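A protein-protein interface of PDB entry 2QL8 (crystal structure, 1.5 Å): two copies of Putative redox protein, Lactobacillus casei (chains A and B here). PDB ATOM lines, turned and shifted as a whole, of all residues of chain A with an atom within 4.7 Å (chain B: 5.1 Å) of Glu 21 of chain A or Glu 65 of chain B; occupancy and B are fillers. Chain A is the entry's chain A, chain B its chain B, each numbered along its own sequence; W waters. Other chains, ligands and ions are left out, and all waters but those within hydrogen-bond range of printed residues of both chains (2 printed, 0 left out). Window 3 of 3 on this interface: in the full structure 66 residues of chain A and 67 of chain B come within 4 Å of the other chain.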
ATOM      1  N   ASP A  19     -31.459   7.129  -7.599  1.00  0.00           N
ATOM      2  CA  ASP A  19     -32.400   7.655  -6.614  1.00  0.00           C
ATOM      3  C   ASP A  19     -32.446   6.872  -5.306  1.00  0.00           C
ATOM      4  O   ASP A  19     -33.422   6.967  -4.538  1.00  0.00           O
ATOM      5  CB  ASP A  19     -33.751   7.791  -7.275  1.00  0.00           C
ATOM      6  CG  ASP A  19     -34.365   6.489  -7.710  1.00  0.00           C
ATOM      7  OD1 ASP A  19     -33.869   5.383  -7.413  1.00  0.00           O
ATOM      8  OD2 ASP A  19     -35.412   6.574  -8.369  1.00  0.00           O
ATOM      9  N   GLU A  20     -31.340   6.214  -4.996  1.00  0.00           N
ATOM     10  CA  GLU A  20     -31.224   5.390  -3.804  1.00  0.00           C
ATOM     11  C   GLU A  20     -30.136   5.809  -2.831  1.00  0.00           C
ATOM     12  O   GLU A  20     -29.408   6.756  -3.070  1.00  0.00           O
ATOM     13  CB  GLU A  20     -31.062   3.901  -4.224  1.00  0.00           C
ATOM     14  CG  GLU A  20     -32.233   3.335  -5.010  1.00  0.00           C
ATOM     15  CD  GLU A  20     -32.007   1.919  -5.524  1.00  0.00           C
ATOM     16  OE1 GLU A  20     -31.453   1.081  -4.782  1.00  0.00           O
ATOM     17  OE2 GLU A  20     -32.355   1.653  -6.692  1.00  0.00           O
ATOM     18  N   GLU A  21     -30.120   5.152  -1.653  1.00  0.00           N
ATOM     19  CA  GLU A  21     -29.095   5.338  -0.641  1.00  0.00           C
ATOM     20  C   GLU A  21     -27.737   4.850  -1.146  1.00  0.00           C
ATOM     21  O   GLU A  21     -27.672   4.159  -2.183  1.00  0.00           O
ATOM     22  CB  GLU A  21     -29.467   4.553   0.656  1.00  0.00           C
ATOM     23  CG  GLU A  21     -30.685   5.107   1.317  1.00  0.00           C
ATOM     24  CD  GLU A  21     -31.226   4.195   2.427  1.00  0.00           C
ATOM     25  OE1 GLU A  21     -31.353   2.959   2.197  1.00  0.00           O
ATOM     26  OE2 GLU A  21     -31.531   4.751   3.497  1.00  0.00           O
ATOM     27  N   LEU A  22     -26.676   5.181  -0.395  1.00  0.00           N
ATOM     28  CA  LEU A  22     -25.307   4.846  -0.788  1.00  0.00           C
ATOM     29  C   LEU A  22     -25.227   3.354  -1.136  1.00  0.00           C
ATOM     30  O   LEU A  22     -24.633   2.951  -2.136  1.00  0.00           O
ATOM     31  CB  LEU A  22     -24.326   5.285   0.311  1.00  0.00           C
ATOM     32  CG  LEU A  22     -22.821   5.219   0.062  1.00  0.00           C
ATOM     33  CD1 LEU A  22     -22.392   5.982  -1.214  1.00  0.00           C
ATOM     34  CD2 LEU A  22     -22.063   5.748   1.333  1.00  0.00           C
ATOM     35  N   GLU A  23     -25.844   2.527  -0.301  1.00  0.00           N
ATOM     36  CA  GLU A  23     -26.033   1.143  -0.646  1.00  0.00           C
ATOM     37  C   GLU A  23     -27.302   1.055  -1.491  1.00  0.00           C
ATOM     38  O   GLU A  23     -28.439   1.063  -0.991  1.00  0.00           O
ATOM     39  CB  GLU A  23     -26.093   0.298   0.627  1.00  0.00           C
ATOM     40  CG  GLU A  23     -24.926   0.593   1.531  1.00  0.00           C
ATOM     41  CD  GLU A  23     -23.582   0.236   0.929  1.00  0.00           C
ATOM     42  OE1 GLU A  23     -23.498  -0.875   0.368  1.00  0.00           O
ATOM     43  OE2 GLU A  23     -22.625   1.016   1.095  1.00  0.00           O
ATOM     44  N   GLY A  24     -27.115   1.062  -2.819  1.00  0.00           N
ATOM     45  CA  GLY A  24     -28.249   1.118  -3.721  1.00  0.00           C
ATOM     46  C   GLY A  24     -27.950   0.601  -5.108  1.00  0.00           C
ATOM     47  O   GLY A  24     -27.397  -0.480  -5.270  1.00  0.00           O
ATOM     48  N   LEU B  60     -23.207  12.320  -7.389  1.00  0.00           N
ATOM     49  CA  LEU B  60     -24.053  13.430  -6.997  1.00  0.00           C
ATOM     50  C   LEU B  60     -25.058  12.971  -5.918  1.00  0.00           C
ATOM     51  O   LEU B  60     -25.322  13.675  -4.946  1.00  0.00           O
ATOM     52  CB  LEU B  60     -24.787  14.049  -8.198  1.00  0.00           C
ATOM     53  CG  LEU B  60     -23.974  15.037  -9.013  1.00  0.00           C
ATOM     54  CD1 LEU B  60     -24.700  15.279 -10.399  1.00  0.00           C
ATOM     55  CD2 LEU B  60     -23.631  16.340  -8.296  1.00  0.00           C
ATOM     56  N   GLU B  61     -25.660  11.819  -6.122  1.00  0.00           N
ATOM     57  CA  GLU B  61     -26.657  11.275  -5.199  1.00  0.00           C
ATOM     58  C   GLU B  61     -26.058  10.993  -3.824  1.00  0.00           C
ATOM     59  O   GLU B  61     -26.661  11.344  -2.798  1.00  0.00           O
ATOM     60  CB  GLU B  61     -27.318  10.032  -5.779  1.00  0.00           C
ATOM     61  CG  GLU B  61     -28.439   9.427  -4.935  1.00  0.00           C
ATOM     62  CD  GLU B  61     -29.761  10.182  -4.885  1.00  0.00           C
ATOM     63  OE1 GLU B  61     -29.848  11.374  -5.267  1.00  0.00           O
ATOM     64  OE2 GLU B  61     -30.769   9.518  -4.458  1.00  0.00           O
ATOM     65  N   ALA B  62     -24.834  10.436  -3.819  1.00  0.00           N
ATOM     66  CA  ALA B  62     -24.119  10.180  -2.549  1.00  0.00           C
ATOM     67  C   ALA B  62     -23.815  11.498  -1.812  1.00  0.00           C
ATOM     68  O   ALA B  62     -23.930  11.609  -0.567  1.00  0.00           O
ATOM     69  CB  ALA B  62     -22.832   9.375  -2.816  1.00  0.00           C
ATOM     70  N   THR B  63     -23.397  12.502  -2.582  1.00  0.00           N
ATOM     71  CA  THR B  63     -23.051  13.825  -2.021  1.00  0.00           C
ATOM     72  C   THR B  63     -24.328  14.461  -1.441  1.00  0.00           C
ATOM     73  O   THR B  63     -24.309  15.031  -0.346  1.00  0.00           O
ATOM     74  CB  THR B  63     -22.382  14.757  -3.078  1.00  0.00           C
ATOM     75  OG1 THR B  63     -21.286  14.053  -3.705  1.00  0.00           O
ATOM     76  CG2 THR B  63     -21.884  16.076  -2.449  1.00  0.00           C
ATOM     77  N   LEU B  64     -25.433  14.347  -2.184  1.00  0.00           N
ATOM     78  CA  LEU B  64     -26.730  14.867  -1.783  1.00  0.00           C
ATOM     79  C   LEU B  64     -27.190  14.222  -0.468  1.00  0.00           C
ATOM     80  O   LEU B  64     -27.704  14.913   0.409  1.00  0.00           O
ATOM     81  CB  LEU B  64     -27.756  14.675  -2.889  1.00  0.00           C
ATOM     82  CG  LEU B  64     -29.166  15.258  -2.670  1.00  0.00           C
ATOM     83  CD1 LEU B  64     -29.170  16.752  -2.289  1.00  0.00           C
ATOM     84  CD2 LEU B  64     -29.992  14.985  -3.940  1.00  0.00           C
ATOM     85  N   GLU B  65     -26.995  12.913  -0.334  1.00  0.00           N
ATOM     86  CA  GLU B  65     -27.363  12.155   0.870  1.00  0.00           C
ATOM     87  C   GLU B  65     -26.598  12.775   2.078  1.00  0.00           C
ATOM     88  O   GLU B  65     -27.181  12.983   3.166  1.00  0.00           O
ATOM     89  CB  GLU B  65     -27.060  10.674   0.653  1.00  0.00           C
ATOM     90  CG  GLU B  65     -27.626   9.790   1.639  1.00  0.00           C
ATOM     91  CD  GLU B  65     -27.378   8.312   1.333  1.00  0.00           C
ATOM     92  OE1 GLU B  65     -26.660   7.968   0.380  1.00  0.00           O
ATOM     93  OE2 GLU B  65     -27.949   7.512   2.092  1.00  0.00           O
ATOM     94  N   ALA B  66     -25.306  13.102   1.899  1.00  0.00           N
ATOM     95  CA  ALA B  66     -24.503  13.746   2.969  1.00  0.00           C
ATOM     96  C   ALA B  66     -25.035  15.137   3.319  1.00  0.00           C
ATOM     97  O   ALA B  66     -25.181  15.493   4.488  1.00  0.00           O
ATOM     98  CB  ALA B  66     -23.012  13.814   2.575  1.00  0.00           C
ATOM     99  N   VAL B  67     -25.392  15.914   2.301  1.00  0.00           N
ATOM    100  CA  VAL B  67     -25.901  17.272   2.506  1.00  0.00           C
ATOM    101  C   VAL B  67     -27.263  17.228   3.197  1.00  0.00           C
ATOM    102  O   VAL B  67     -27.526  18.016   4.101  1.00  0.00           O
ATOM    103  CB  VAL B  67     -25.956  18.044   1.145  1.00  0.00           C
ATOM    104  CG1 VAL B  67     -26.824  19.349   1.231  1.00  0.00           C
ATOM    105  CG2 VAL B  67     -24.535  18.389   0.686  1.00  0.00           C
ATOM    106  N   GLU B  68     -28.131  16.310   2.795  1.00  0.00           N
ATOM    107  CA  GLU B  68     -29.425  16.189   3.450  1.00  0.00           C
ATOM    108  C   GLU B  68     -29.237  15.922   4.945  1.00  0.00           C
ATOM    109  O   GLU B  68     -29.900  16.536   5.790  1.00  0.00           O
ATOM    110  CB  GLU B  68     -30.261  15.078   2.811  1.00  0.00           C
ATOM    111  CG  GLU B  68     -30.794  15.432   1.395  1.00  0.00           C
ATOM    112  CD  GLU B  68     -31.271  14.197   0.658  1.00  0.00           C
ATOM    113  OE1 GLU B  68     -30.506  13.185   0.675  1.00  0.00           O
ATOM    114  OE2 GLU B  68     -32.372  14.221   0.062  1.00  0.00           O
ATOM    115  N   LYS B  69     -28.352  14.967   5.239  1.00  0.00           N
ATOM    116  CA  LYS B  69     -28.074  14.589   6.625  1.00  0.00           C
ATOM    117  C   LYS B  69     -27.529  15.783   7.427  1.00  0.00           C
ATOM    118  O   LYS B  69     -27.909  15.994   8.584  1.00  0.00           O
ATOM    119  CB  LYS B  69     -27.103  13.400   6.646  1.00  0.00           C
ATOM    120  CG  LYS B  69     -26.542  12.991   8.016  1.00  0.00           C
ATOM    121  CD  LYS B  69     -27.566  12.375   8.880  1.00  0.00           C
ATOM    122  CE  LYS B  69     -28.032  11.002   8.389  1.00  0.00           C
ATOM    123  NZ  LYS B  69     -26.957   9.948   8.569  1.00  0.00           N
ATOM    124  N   HIS B  75     -33.325  11.253   3.371  1.00  0.00           N
ATOM    125  CA  HIS B  75     -32.900  11.143   1.977  1.00  0.00           C
ATOM    126  C   HIS B  75     -34.092  11.017   1.031  1.00  0.00           C
ATOM    127  O   HIS B  75     -34.694   9.948   0.972  1.00  0.00           O
ATOM    128  CB  HIS B  75     -31.933   9.969   1.790  1.00  0.00           C
ATOM    129  CG  HIS B  75     -31.408   9.852   0.397  1.00  0.00           C
ATOM    130  ND1 HIS B  75     -31.002  10.951  -0.334  1.00  0.00           N
ATOM    131  CD2 HIS B  75     -31.221   8.762  -0.389  1.00  0.00           C
ATOM    132  CE1 HIS B  75     -30.566  10.529  -1.508  1.00  0.00           C
ATOM    133  NE2 HIS B  75     -30.691   9.208  -1.570  1.00  0.00           N
HETATM  134  O   HOH W   1     -33.667   6.717   1.745  1.00  0.00           O
HETATM  135  O   HOH W   2     -26.807   7.768  -2.464  1.00  0.00           O
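OE1 of Glu 65 of chain B sits at hydrogen-bond distance from N of Leu 22 of chain A (2.9 Å). N of Glu 20 of chain A lies within hydrogen-bond range of OE2 of Glu 61 of chain B (3.4 Å). NE2 of His 75 of chain B lies within hydrogen-bond range of O of Glu 20 of chain A.
A ring nitrogen (ND1) of His 75 of chain B sits at hydrogen-bond distance from the side-chain carboxylate (OE1) of Glu 68 of chain B (2.5 Å). The side-chain carboxylate of Glu 61 of chain B is in hydrogen-bond range of a ring nitrogen (NE2) of His 75 of chain B, at 2.9 Å.
Among the printed residues, merely in contact across the chains: Asp 19 of chain A with Glu 61 of chain B (3.2 Å), Glu 21 of chain A with Glu 65 of chain B (3.6 Å), Glu 21 of chain A with His 75 of chain B (3.98 Å) and Leu 22 of chain A with Ala 62 of chain B (3.8 Å).
Printed residues of chain B within 4 Å of Asp 19 of chain A: Glu 61. Printed residues of chain B within 4 Å of Glu 20 of chain A: Glu 61 and His 75. Printed residues of chain B within 4 Å of Glu 21 of chain A: Glu 65 and His 75. Printed residues of chain B within 4 Å of Leu 22 of chain A: Ala 62 (3.8 Å) and Glu 65 (2.9 Å). Of the printed residues of chain A, Ala 62 of chain B touches Leu 22 (3.8 Å). Glu 65 of chain B touches just these residues of chain A: Glu 21 and Leu 22. Lys 69 of chain B touches none of the printed residues of chain A. Of the printed residues of chain A, His 75 of chain B touches Glu 20 and Glu 21. The nearest printed residue of chain A that does not touch Ala 62 of chain B is Glu 20 of chain A (5.9 Å).
Hydrophobic or aromatic side chains of chain A that line the printed part of chain B: Leu 22. Hydrophobic or aromatic side chains of chain B that line the printed part of chain A: Ala 62 and His 75.
No position is printed for both chains.
Water W2 lies within hydrogen-bond range of the side-chain carboxylate (OE1) of Glu 65 of chain B, the backbone carbonyl oxygen (O) of Glu 20 of chain A and the backbone NH (N) of Leu 22 of chain A. Water W1 lies within hydrogen-bond range of OE2 of Glu 21 of chain A (3.4 Å) and O of His 75 of chain B (3.5 Å).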
